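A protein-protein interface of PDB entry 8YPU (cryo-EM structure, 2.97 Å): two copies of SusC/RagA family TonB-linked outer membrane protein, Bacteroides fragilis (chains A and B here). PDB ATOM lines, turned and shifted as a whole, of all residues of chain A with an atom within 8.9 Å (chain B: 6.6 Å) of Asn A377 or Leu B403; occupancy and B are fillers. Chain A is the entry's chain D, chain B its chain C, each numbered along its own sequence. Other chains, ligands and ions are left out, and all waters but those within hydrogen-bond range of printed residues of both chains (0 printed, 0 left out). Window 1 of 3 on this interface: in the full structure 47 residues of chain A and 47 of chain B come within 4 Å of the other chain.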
ATOM      1  N   GLY A 109      15.389  -6.714   1.699  1.00  0.00           N
ATOM      2  CA  GLY A 109      14.406  -7.727   1.388  1.00  0.00           C
ATOM      3  C   GLY A 109      13.036  -7.208   1.023  1.00  0.00           C
ATOM      4  O   GLY A 109      12.117  -8.006   0.827  1.00  0.00           O
ATOM      5  N   LEU A 285      14.150 -13.270  -4.282  1.00  0.00           N
ATOM      6  CA  LEU A 285      12.788 -13.701  -4.556  1.00  0.00           C
ATOM      7  C   LEU A 285      11.946 -13.412  -3.329  1.00  0.00           C
ATOM      8  O   LEU A 285      12.300 -13.824  -2.225  1.00  0.00           O
ATOM      9  CB  LEU A 285      12.736 -15.192  -4.894  1.00  0.00           C
ATOM     10  CG  LEU A 285      11.363 -15.863  -4.912  1.00  0.00           C
ATOM     11  CD1 LEU A 285      10.546 -15.384  -6.089  1.00  0.00           C
ATOM     12  CD2 LEU A 285      11.512 -17.365  -4.941  1.00  0.00           C
ATOM     13  N   PHE A 306       5.319 -10.836   4.654  1.00  0.00           N
ATOM     14  CA  PHE A 306       6.399 -10.520   3.729  1.00  0.00           C
ATOM     15  C   PHE A 306       7.475 -11.577   3.911  1.00  0.00           C
ATOM     16  O   PHE A 306       8.183 -11.566   4.921  1.00  0.00           O
ATOM     17  CB  PHE A 306       6.986  -9.132   3.988  1.00  0.00           C
ATOM     18  CG  PHE A 306       5.967  -8.054   4.192  1.00  0.00           C
ATOM     19  CD1 PHE A 306       5.419  -7.828   5.439  1.00  0.00           C
ATOM     20  CD2 PHE A 306       5.592  -7.236   3.150  1.00  0.00           C
ATOM     21  CE1 PHE A 306       4.494  -6.835   5.629  1.00  0.00           C
ATOM     22  CE2 PHE A 306       4.668  -6.238   3.341  1.00  0.00           C
ATOM     23  CZ  PHE A 306       4.121  -6.040   4.580  1.00  0.00           C
ATOM     24  N   VAL A 307       7.602 -12.493   2.959  1.00  0.00           N
ATOM     25  CA  VAL A 307       8.665 -13.486   3.006  1.00  0.00           C
ATOM     26  C   VAL A 307       9.646 -13.178   1.889  1.00  0.00           C
ATOM     27  O   VAL A 307       9.274 -12.670   0.829  1.00  0.00           O
ATOM     28  CB  VAL A 307       8.143 -14.935   2.913  1.00  0.00           C
ATOM     29  CG1 VAL A 307       7.338 -15.277   4.141  1.00  0.00           C
ATOM     30  CG2 VAL A 307       7.304 -15.126   1.691  1.00  0.00           C
ATOM     31  N   ASN A 308      10.914 -13.479   2.141  1.00  0.00           N
ATOM     32  CA  ASN A 308      11.994 -13.000   1.296  1.00  0.00           C
ATOM     33  C   ASN A 308      13.136 -14.005   1.326  1.00  0.00           C
ATOM     34  O   ASN A 308      13.394 -14.639   2.352  1.00  0.00           O
ATOM     35  CB  ASN A 308      12.445 -11.618   1.776  1.00  0.00           C
ATOM     36  CG  ASN A 308      13.814 -11.262   1.310  1.00  0.00           C
ATOM     37  OD1 ASN A 308      14.729 -11.080   2.106  1.00  0.00           O
ATOM     38  ND2 ASN A 308      13.968 -11.139   0.002  1.00  0.00           N
ATOM     39  N   ARG A 309      13.814 -14.154   0.193  1.00  0.00           N
ATOM     40  CA  ARG A 309      14.971 -15.035   0.109  1.00  0.00           C
ATOM     41  C   ARG A 309      15.986 -14.426  -0.842  1.00  0.00           C
ATOM     42  O   ARG A 309      15.692 -14.254  -2.027  1.00  0.00           O
ATOM     43  CB  ARG A 309      14.573 -16.422  -0.368  1.00  0.00           C
ATOM     44  CG  ARG A 309      15.741 -17.358  -0.477  1.00  0.00           C
ATOM     45  CD  ARG A 309      15.323 -18.702  -0.985  1.00  0.00           C
ATOM     46  NE  ARG A 309      16.005 -19.764  -0.261  1.00  0.00           N
ATOM     47  CZ  ARG A 309      17.075 -20.402  -0.708  1.00  0.00           C
ATOM     48  NH1 ARG A 309      17.599 -20.125  -1.891  1.00  0.00           N
ATOM     49  NH2 ARG A 309      17.636 -21.336   0.053  1.00  0.00           N
ATOM     50  N   ARG A 310      17.172 -14.116  -0.332  1.00  0.00           N
ATOM     51  CA  ARG A 310      18.233 -13.500  -1.116  1.00  0.00           C
ATOM     52  C   ARG A 310      19.459 -14.397  -1.112  1.00  0.00           C
ATOM     53  O   ARG A 310      19.921 -14.816  -0.051  1.00  0.00           O
ATOM     54  CB  ARG A 310      18.598 -12.118  -0.570  1.00  0.00           C
ATOM     55  CG  ARG A 310      17.423 -11.347  -0.026  1.00  0.00           C
ATOM     56  CD  ARG A 310      17.757  -9.894   0.152  1.00  0.00           C
ATOM     57  NE  ARG A 310      18.553  -9.644   1.346  1.00  0.00           N
ATOM     58  CZ  ARG A 310      18.053  -9.537   2.568  1.00  0.00           C
ATOM     59  NH1 ARG A 310      16.768  -9.724   2.807  1.00  0.00           N
ATOM     60  NH2 ARG A 310      18.862  -9.232   3.576  1.00  0.00           N
ATOM     61  N   ASN A 311      19.986 -14.683  -2.295  1.00  0.00           N
ATOM     62  CA  ASN A 311      21.192 -15.483  -2.452  1.00  0.00           C
ATOM     63  C   ASN A 311      22.292 -14.610  -3.033  1.00  0.00           C
ATOM     64  O   ASN A 311      22.134 -14.055  -4.124  1.00  0.00           O
ATOM     65  CB  ASN A 311      20.931 -16.691  -3.347  1.00  0.00           C
ATOM     66  CG  ASN A 311      21.731 -17.901  -2.931  1.00  0.00           C
ATOM     67  OD1 ASN A 311      22.926 -17.805  -2.645  1.00  0.00           O
ATOM     68  ND2 ASN A 311      21.074 -19.052  -2.887  1.00  0.00           N
ATOM     69  N   GLU A 374      26.295 -16.634   0.475  1.00  0.00           N
ATOM     70  CA  GLU A 374      25.393 -16.344   1.578  1.00  0.00           C
ATOM     71  C   GLU A 374      23.945 -16.486   1.135  1.00  0.00           C
ATOM     72  O   GLU A 374      23.607 -16.241  -0.022  1.00  0.00           O
ATOM     73  CB  GLU A 374      25.618 -14.945   2.136  1.00  0.00           C
ATOM     74  CG  GLU A 374      25.291 -14.837   3.601  1.00  0.00           C
ATOM     75  CD  GLU A 374      25.249 -13.415   4.077  1.00  0.00           C
ATOM     76  OE1 GLU A 374      25.161 -12.505   3.227  1.00  0.00           O
ATOM     77  OE2 GLU A 374      25.301 -13.203   5.304  1.00  0.00           O
ATOM     78  N   THR A 375      23.093 -16.896   2.073  1.00  0.00           N
ATOM     79  CA  THR A 375      21.659 -17.024   1.839  1.00  0.00           C
ATOM     80  C   THR A 375      20.916 -16.411   3.012  1.00  0.00           C
ATOM     81  O   THR A 375      21.127 -16.815   4.156  1.00  0.00           O
ATOM     82  CB  THR A 375      21.245 -18.485   1.664  1.00  0.00           C
ATOM     83  OG1 THR A 375      22.132 -19.126   0.741  1.00  0.00           O
ATOM     84  CG2 THR A 375      19.836 -18.571   1.133  1.00  0.00           C
ATOM     85  N   ILE A 376      20.039 -15.455   2.729  1.00  0.00           N
ATOM     86  CA  ILE A 376      19.247 -14.772   3.742  1.00  0.00           C
ATOM     87  C   ILE A 376      17.790 -15.147   3.540  1.00  0.00           C
ATOM     88  O   ILE A 376      17.213 -14.875   2.482  1.00  0.00           O
ATOM     89  CB  ILE A 376      19.427 -13.250   3.677  1.00  0.00           C
ATOM     90  CG1 ILE A 376      20.906 -12.880   3.695  1.00  0.00           C
ATOM     91  CG2 ILE A 376      18.717 -12.606   4.828  1.00  0.00           C
ATOM     92  CD1 ILE A 376      21.391 -12.253   2.426  1.00  0.00           C
ATOM     93  N   ASN A 377      17.199 -15.765   4.556  1.00  0.00           N
ATOM     94  CA  ASN A 377      15.786 -16.113   4.584  1.00  0.00           C
ATOM     95  C   ASN A 377      15.102 -15.221   5.609  1.00  0.00           C
ATOM     96  O   ASN A 377      15.436 -15.267   6.794  1.00  0.00           O
ATOM     97  CB  ASN A 377      15.600 -17.587   4.943  1.00  0.00           C
ATOM     98  CG  ASN A 377      15.918 -18.512   3.794  1.00  0.00           C
ATOM     99  OD1 ASN A 377      15.103 -18.701   2.898  1.00  0.00           O
ATOM    100  ND2 ASN A 377      17.102 -19.102   3.816  1.00  0.00           N
ATOM    101  N   ALA A 378      14.150 -14.413   5.160  1.00  0.00           N
ATOM    102  CA  ALA A 378      13.526 -13.417   6.013  1.00  0.00           C
ATOM    103  C   ALA A 378      12.016 -13.575   5.993  1.00  0.00           C
ATOM    104  O   ALA A 378      11.428 -13.871   4.953  1.00  0.00           O
ATOM    105  CB  ALA A 378      13.904 -12.009   5.571  1.00  0.00           C
ATOM    106  N   LEU A 379      11.399 -13.383   7.151  1.00  0.00           N
ATOM    107  CA  LEU A 379       9.955 -13.391   7.299  1.00  0.00           C
ATOM    108  C   LEU A 379       9.550 -12.208   8.159  1.00  0.00           C
ATOM    109  O   LEU A 379      10.241 -11.866   9.118  1.00  0.00           O
ATOM    110  CB  LEU A 379       9.456 -14.693   7.937  1.00  0.00           C
ATOM    111  CG  LEU A 379       7.946 -14.858   8.112  1.00  0.00           C
ATOM    112  CD1 LEU A 379       7.528 -16.223   7.647  1.00  0.00           C
ATOM    113  CD2 LEU A 379       7.528 -14.641   9.556  1.00  0.00           C
ATOM    114  N   SER A 380       8.433 -11.581   7.809  1.00  0.00           N
ATOM    115  CA  SER A 380       7.909 -10.470   8.597  1.00  0.00           C
ATOM    116  C   SER A 380       6.392 -10.519   8.518  1.00  0.00           C
ATOM    117  O   SER A 380       5.820 -10.314   7.449  1.00  0.00           O
ATOM    118  CB  SER A 380       8.451  -9.140   8.088  1.00  0.00           C
ATOM    119  OG  SER A 380       8.268  -8.113   9.041  1.00  0.00           O
ATOM    120  N   GLN A 402       9.229 -10.917  13.382  1.00  0.00           N
ATOM    121  CA  GLN A 402      10.250 -10.755  12.364  1.00  0.00           C
ATOM    122  C   GLN A 402      11.347 -11.776  12.590  1.00  0.00           C
ATOM    123  O   GLN A 402      11.811 -11.949  13.717  1.00  0.00           O
ATOM    124  CB  GLN A 402      10.840  -9.347  12.388  1.00  0.00           C
ATOM    125  CG  GLN A 402      11.758  -9.061  11.230  1.00  0.00           C
ATOM    126  CD  GLN A 402      12.299  -7.664  11.263  1.00  0.00           C
ATOM    127  OE1 GLN A 402      11.869  -6.845  12.069  1.00  0.00           O
ATOM    128  NE2 GLN A 402      13.248  -7.376  10.387  1.00  0.00           N
ATOM    129  N   LEU A 403      11.759 -12.436  11.517  1.00  0.00           N
ATOM    130  CA  LEU A 403      12.838 -13.405  11.550  1.00  0.00           C
ATOM    131  C   LEU A 403      13.750 -13.141  10.366  1.00  0.00           C
ATOM    132  O   LEU A 403      13.272 -12.846   9.271  1.00  0.00           O
ATOM    133  CB  LEU A 403      12.290 -14.832  11.504  1.00  0.00           C
ATOM    134  CG  LEU A 403      13.286 -15.984  11.518  1.00  0.00           C
ATOM    135  CD1 LEU A 403      13.733 -16.290  12.931  1.00  0.00           C
ATOM    136  CD2 LEU A 403      12.653 -17.191  10.878  1.00  0.00           C
ATOM    137  N   ASP A 404      15.057 -13.233  10.583  1.00  0.00           N
ATOM    138  CA  ASP A 404      16.019 -12.999   9.510  1.00  0.00           C
ATOM    139  C   ASP A 404      17.216 -13.905   9.749  1.00  0.00           C
ATOM    140  O   ASP A 404      17.986 -13.668  10.681  1.00  0.00           O
ATOM    141  CB  ASP A 404      16.434 -11.534   9.471  1.00  0.00           C
ATOM    142  CG  ASP A 404      17.029 -11.131   8.143  1.00  0.00           C
ATOM    143  OD1 ASP A 404      17.968 -11.809   7.684  1.00  0.00           O
ATOM    144  OD2 ASP A 404      16.568 -10.128   7.559  1.00  0.00           O
ATOM    145  N   LYS A 405      17.377 -14.934   8.922  1.00  0.00           N
ATOM    146  CA  LYS A 405      18.430 -15.929   9.097  1.00  0.00           C
ATOM    147  C   LYS A 405      19.393 -15.854   7.921  1.00  0.00           C
ATOM    148  O   LYS A 405      19.009 -16.132   6.783  1.00  0.00           O
ATOM    149  CB  LYS A 405      17.834 -17.327   9.211  1.00  0.00           C
ATOM    150  CG  LYS A 405      16.761 -17.456  10.264  1.00  0.00           C
ATOM    151  CD  LYS A 405      16.137 -18.831  10.234  1.00  0.00           C
ATOM    152  CE  LYS A 405      17.156 -19.905  10.538  1.00  0.00           C
ATOM    153  NZ  LYS A 405      17.635 -19.841  11.938  1.00  0.00           N
ATOM    154  N   ALA A 406      20.643 -15.498   8.197  1.00  0.00           N
ATOM    155  CA  ALA A 406      21.692 -15.438   7.191  1.00  0.00           C
ATOM    156  C   ALA A 406      22.658 -16.590   7.409  1.00  0.00           C
ATOM    157  O   ALA A 406      23.191 -16.761   8.506  1.00  0.00           O
ATOM    158  CB  ALA A 406      22.434 -14.106   7.253  1.00  0.00           C
ATOM    159  N   SER A 407      22.876 -17.378   6.364  1.00  0.00           N
ATOM    160  CA  SER A 407      23.782 -18.519   6.395  1.00  0.00           C
ATOM    161  C   SER A 407      24.874 -18.272   5.368  1.00  0.00           C
ATOM    162  O   SER A 407      24.603 -18.253   4.164  1.00  0.00           O
ATOM    163  CB  SER A 407      23.038 -19.816   6.102  1.00  0.00           C
ATOM    164  OG  SER A 407      22.178 -20.155   7.171  1.00  0.00           O
ATOM    165  N   GLU A 450      26.222 -18.683  10.798  1.00  0.00           N
ATOM    166  CA  GLU A 450      24.763 -18.693  10.891  1.00  0.00           C
ATOM    167  C   GLU A 450      24.345 -17.594  11.857  1.00  0.00           C
ATOM    168  O   GLU A 450      24.558 -17.727  13.062  1.00  0.00           O
ATOM    169  CB  GLU A 450      24.239 -20.050  11.365  1.00  0.00           C
ATOM    170  CG  GLU A 450      24.906 -21.256  10.732  1.00  0.00           C
ATOM    171  CD  GLU A 450      24.316 -21.620   9.385  1.00  0.00           C
ATOM    172  OE1 GLU A 450      23.075 -21.685   9.276  1.00  0.00           O
ATOM    173  OE2 GLU A 450      25.093 -21.846   8.434  1.00  0.00           O
ATOM    174  N   ASN A 451      23.753 -16.519  11.341  1.00  0.00           N
ATOM    175  CA  ASN A 451      23.318 -15.384  12.149  1.00  0.00           C
ATOM    176  C   ASN A 451      21.805 -15.257  12.059  1.00  0.00           C
ATOM    177  O   ASN A 451      21.259 -15.102  10.966  1.00  0.00           O
ATOM    178  CB  ASN A 451      23.983 -14.088  11.683  1.00  0.00           C
ATOM    179  CG  ASN A 451      25.433 -14.278  11.307  1.00  0.00           C
ATOM    180  OD1 ASN A 451      26.299 -14.393  12.171  1.00  0.00           O
ATOM    181  ND2 ASN A 451      25.709 -14.313  10.012  1.00  0.00           N
ATOM    182  N   THR A 452      21.132 -15.297  13.204  1.00  0.00           N
ATOM    183  CA  THR A 452      19.679 -15.211  13.277  1.00  0.00           C
ATOM    184  C   THR A 452      19.294 -13.979  14.079  1.00  0.00           C
ATOM    185  O   THR A 452      19.732 -13.818  15.223  1.00  0.00           O
ATOM    186  CB  THR A 452      19.088 -16.464  13.918  1.00  0.00           C
ATOM    187  OG1 THR A 452      19.681 -17.625  13.328  1.00  0.00           O
ATOM    188  CG2 THR A 452      17.591 -16.513  13.709  1.00  0.00           C
ATOM    189  N   ASN A 453      18.476 -13.119  13.483  1.00  0.00           N
ATOM    190  CA  ASN A 453      17.936 -11.939  14.143  1.00  0.00           C
ATOM    191  C   ASN A 453      16.426 -12.098  14.221  1.00  0.00           C
ATOM    192  O   ASN A 453      15.754 -12.158  13.189  1.00  0.00           O
ATOM    193  CB  ASN A 453      18.316 -10.672  13.377  1.00  0.00           C
ATOM    194  CG  ASN A 453      18.423  -9.460  14.268  1.00  0.00           C
ATOM    195  OD1 ASN A 453      17.748  -9.362  15.290  1.00  0.00           O
ATOM    196  ND2 ASN A 453      19.288  -8.530  13.892  1.00  0.00           N
ATOM    197  N   ASN B 377      11.914 -23.910  11.246  1.00  0.00           N
ATOM    198  CA  ASN B 377      11.285 -22.844  10.480  1.00  0.00           C
ATOM    199  C   ASN B 377      10.969 -23.387   9.094  1.00  0.00           C
ATOM    200  O   ASN B 377      11.877 -23.785   8.361  1.00  0.00           O
ATOM    201  CB  ASN B 377      12.206 -21.629  10.385  1.00  0.00           C
ATOM    202  CG  ASN B 377      12.250 -20.829  11.664  1.00  0.00           C
ATOM    203  OD1 ASN B 377      11.354 -20.039  11.938  1.00  0.00           O
ATOM    204  ND2 ASN B 377      13.297 -21.020  12.449  1.00  0.00           N
ATOM    205  N   ALA B 378       9.692 -23.401   8.731  1.00  0.00           N
ATOM    206  CA  ALA B 378       9.256 -24.025   7.495  1.00  0.00           C
ATOM    207  C   ALA B 378       8.437 -23.047   6.670  1.00  0.00           C
ATOM    208  O   ALA B 378       7.654 -22.267   7.211  1.00  0.00           O
ATOM    209  CB  ALA B 378       8.434 -25.276   7.777  1.00  0.00           C
ATOM    210  N   LEU B 379       8.632 -23.093   5.358  1.00  0.00           N
ATOM    211  CA  LEU B 379       7.864 -22.309   4.409  1.00  0.00           C
ATOM    212  C   LEU B 379       7.456 -23.208   3.256  1.00  0.00           C
ATOM    213  O   LEU B 379       8.230 -24.065   2.827  1.00  0.00           O
ATOM    214  CB  LEU B 379       8.665 -21.114   3.879  1.00  0.00           C
ATOM    215  CG  LEU B 379       7.965 -20.171   2.900  1.00  0.00           C
ATOM    216  CD1 LEU B 379       8.213 -18.747   3.303  1.00  0.00           C
ATOM    217  CD2 LEU B 379       8.429 -20.406   1.474  1.00  0.00           C
ATOM    218  N   SER B 380       6.241 -23.017   2.759  1.00  0.00           N
ATOM    219  CA  SER B 380       5.764 -23.777   1.609  1.00  0.00           C
ATOM    220  C   SER B 380       4.843 -22.872   0.805  1.00  0.00           C
ATOM    221  O   SER B 380       3.769 -22.504   1.277  1.00  0.00           O
ATOM    222  CB  SER B 380       5.047 -25.046   2.055  1.00  0.00           C
ATOM    223  OG  SER B 380       4.914 -25.962   0.988  1.00  0.00           O
ATOM    224  N   SER B 381       5.259 -22.516  -0.403  1.00  0.00           N
ATOM    225  CA  SER B 381       4.492 -21.635  -1.266  1.00  0.00           C
ATOM    226  C   SER B 381       4.140 -22.353  -2.560  1.00  0.00           C
ATOM    227  O   SER B 381       4.982 -23.026  -3.152  1.00  0.00           O
ATOM    228  CB  SER B 381       5.272 -20.361  -1.576  1.00  0.00           C
ATOM    229  OG  SER B 381       5.879 -20.444  -2.849  1.00  0.00           O
ATOM    230  N   LEU B 401       7.516 -24.130  -3.990  1.00  0.00           N
ATOM    231  CA  LEU B 401       8.772 -23.941  -3.283  1.00  0.00           C
ATOM    232  C   LEU B 401       8.594 -24.372  -1.838  1.00  0.00           C
ATOM    233  O   LEU B 401       7.590 -24.046  -1.206  1.00  0.00           O
ATOM    234  CB  LEU B 401       9.233 -22.485  -3.325  1.00  0.00           C
ATOM    235  CG  LEU B 401       9.102 -21.708  -4.630  1.00  0.00           C
ATOM    236  CD1 LEU B 401       9.041 -20.232  -4.336  1.00  0.00           C
ATOM    237  CD2 LEU B 401      10.264 -22.016  -5.533  1.00  0.00           C
ATOM    238  N   GLN B 402       9.561 -25.115  -1.319  1.00  0.00           N
ATOM    239  CA  GLN B 402       9.489 -25.616   0.042  1.00  0.00           C
ATOM    240  C   GLN B 402      10.841 -25.459   0.704  1.00  0.00           C
ATOM    241  O   GLN B 402      11.865 -25.809   0.116  1.00  0.00           O
ATOM    242  CB  GLN B 402       9.063 -27.082   0.073  1.00  0.00           C
ATOM    243  CG  GLN B 402       8.780 -27.595   1.459  1.00  0.00           C
ATOM    244  CD  GLN B 402       8.335 -29.025   1.458  1.00  0.00           C
ATOM    245  OE1 GLN B 402       8.089 -29.604   0.405  1.00  0.00           O
ATOM    246  NE2 GLN B 402       8.225 -29.611   2.641  1.00  0.00           N
ATOM    247  N   LEU B 403      10.837 -24.942   1.925  1.00  0.00           N
ATOM    248  CA  LEU B 403      12.040 -24.776   2.718  1.00  0.00           C
ATOM    249  C   LEU B 403      11.749 -25.260   4.127  1.00  0.00           C
ATOM    250  O   LEU B 403      10.671 -25.003   4.659  1.00  0.00           O
ATOM    251  CB  LEU B 403      12.488 -23.315   2.727  1.00  0.00           C
ATOM    252  CG  LEU B 403      13.734 -22.951   3.524  1.00  0.00           C
ATOM    253  CD1 LEU B 403      14.985 -23.245   2.726  1.00  0.00           C
ATOM    254  CD2 LEU B 403      13.667 -21.498   3.911  1.00  0.00           C
ATOM    255  N   ASP B 404      12.703 -25.964   4.727  1.00  0.00           N
ATOM    256  CA  ASP B 404      12.523 -26.476   6.082  1.00  0.00           C
ATOM    257  C   ASP B 404      13.879 -26.468   6.769  1.00  0.00           C
ATOM    258  O   ASP B 404      14.742 -27.279   6.427  1.00  0.00           O
ATOM    259  CB  ASP B 404      11.926 -27.877   6.053  1.00  0.00           C
ATOM    260  CG  ASP B 404      11.284 -28.265   7.364  1.00  0.00           C
ATOM    261  OD1 ASP B 404      11.954 -28.153   8.407  1.00  0.00           O
ATOM    262  OD2 ASP B 404      10.112 -28.694   7.352  1.00  0.00           O
ATOM    263  N   LYS B 405      14.075 -25.564   7.726  1.00  0.00           N
ATOM    264  CA  LYS B 405      15.358 -25.391   8.397  1.00  0.00           C
ATOM    265  C   LYS B 405      15.210 -25.753   9.867  1.00  0.00           C
ATOM    266  O   LYS B 405      14.480 -25.085  10.601  1.00  0.00           O
ATOM    267  CB  LYS B 405      15.854 -23.957   8.248  1.00  0.00           C
ATOM    268  CG  LYS B 405      15.897 -23.464   6.824  1.00  0.00           C
ATOM    269  CD  LYS B 405      16.282 -22.005   6.767  1.00  0.00           C
ATOM    270  CE  LYS B 405      17.667 -21.778   7.329  1.00  0.00           C
ATOM    271  NZ  LYS B 405      18.720 -22.380   6.479  1.00  0.00           N
ATOM    272  N   THR B 452      18.977 -28.246   6.576  1.00  0.00           N
ATOM    273  CA  THR B 452      18.106 -27.522   5.661  1.00  0.00           C
ATOM    274  C   THR B 452      17.651 -28.454   4.550  1.00  0.00           C
ATOM    275  O   THR B 452      18.480 -29.056   3.861  1.00  0.00           O
ATOM    276  CB  THR B 452      18.823 -26.313   5.064  1.00  0.00           C
ATOM    277  OG1 THR B 452      19.487 -25.592   6.106  1.00  0.00           O
ATOM    278  CG2 THR B 452      17.835 -25.396   4.380  1.00  0.00           C
ATOM    279  N   ASN B 453      16.339 -28.564   4.376  1.00  0.00           N
ATOM    280  CA  ASN B 453      15.736 -29.340   3.302  1.00  0.00           C
ATOM    281  C   ASN B 453      14.975 -28.380   2.402  1.00  0.00           C
ATOM    282  O   ASN B 453      14.018 -27.741   2.844  1.00  0.00           O
ATOM    283  CB  ASN B 453      14.807 -30.414   3.869  1.00  0.00           C
ATOM    284  CG  ASN B 453      14.712 -31.632   2.985  1.00  0.00           C
ATOM    285  OD1 ASN B 453      14.850 -31.543   1.768  1.00  0.00           O
ATOM    286  ND2 ASN B 453      14.487 -32.783   3.596  1.00  0.00           N
ATOM    287  N   SER B 454      15.403 -28.274   1.149  1.00  0.00           N
ATOM    288  CA  SER B 454      14.794 -27.379   0.180  1.00  0.00           C
ATOM    289  C   SER B 454      14.283 -28.184  -1.004  1.00  0.00           C
ATOM    290  O   SER B 454      14.821 -29.243  -1.328  1.00  0.00           O
ATOM    291  CB  SER B 454      15.786 -26.323  -0.308  1.00  0.00           C
ATOM    292  OG  SER B 454      16.320 -25.580   0.767  1.00  0.00           O
ATOM    293  N   GLN B 455      13.248 -27.666  -1.652  1.00  0.00           N
ATOM    294  CA  GLN B 455      12.677 -28.320  -2.818  1.00  0.00           C
ATOM    295  C   GLN B 455      12.004 -27.281  -3.697  1.00  0.00           C
ATOM    296  O   GLN B 455      11.348 -26.371  -3.195  1.00  0.00           O
ATOM    297  CB  GLN B 455      11.673 -29.392  -2.402  1.00  0.00           C
ATOM    298  CG  GLN B 455      11.503 -30.523  -3.384  1.00  0.00           C
ATOM    299  CD  GLN B 455      10.123 -31.119  -3.322  1.00  0.00           C
ATOM    300  OE1 GLN B 455       9.140 -30.412  -3.135  1.00  0.00           O
ATOM    301  NE2 GLN B 455      10.040 -32.425  -3.468  1.00  0.00           N
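Of the 14 printed residues of chain B, 5 touch a printed residue of chain A. Hydrophobic or aromatic side chains of chain B that line the printed part of chain A: Leu B379, Leu B401 and Leu B403.
Asn A377 touches Leu B403, and with the chains exchanged Leu A403 touches Asn B377. Lys A405 touches its own counterpart, Lys B405. 10 positions are printed for both chains. Of the 5 pairs that touch across the chains among the printed residues, 3 have their exchanged pair printed and touching as well.
Among the printed residues, merely in contact across the chains: Asn A377 with Leu B403 (3.3 Å), Leu A403 with Asn B377 (3.3 Å), Val A307 with Leu B379 (3.7 Å), Lys A405 with Lys B405 (3.8 Å) and Leu A285 with Leu B401 (3.8 Å).
Of the printed residues of chain B, Leu A285 touches Leu B401. Asn A311 touches none of the printed residues of chain B. Of chain B, only Leu B403 (3.3 Å) comes within 4 Å of Asn A377. Gln A402 touches none of the printed residues of chain B. Of the printed residues of chain A, Asn B377 touches Leu A403 (3.3 Å). No residue of chain A comes within 4 Å of Ala B378. Leu B403 touches just one residue of chain A: Asn A377. The nearest printed residue of chain A that does not touch Leu B379 is Leu A379 (5.1 Å).
N of Asn A377 lies within hydrogen-bond range of O of Lys A405, 2.9 Å away. The side-chain amino group (NZ) of Lys A405 sits at hydrogen-bond distance from the side-chain hydroxyl (OG1) of Thr A452 (3.3 Å). The side-chain amino group of Lys B405 lies within hydrogen-bond range of the side-chain hydroxyl of Thr B452 (3.3 Å). O of Ser B381 sits at hydrogen-bond distance from N of Leu B401, at 2.9 Å. The backbone carbonyl oxygen (O) of Leu B403 sits at hydrogen-bond distance from the backbone NH (N) of Leu B379, at 2.9 Å. The backbone NH (N) of Leu A379 lies within hydrogen-bond range of the backbone carbonyl oxygen (O) of Leu A403 (2.9 Å).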
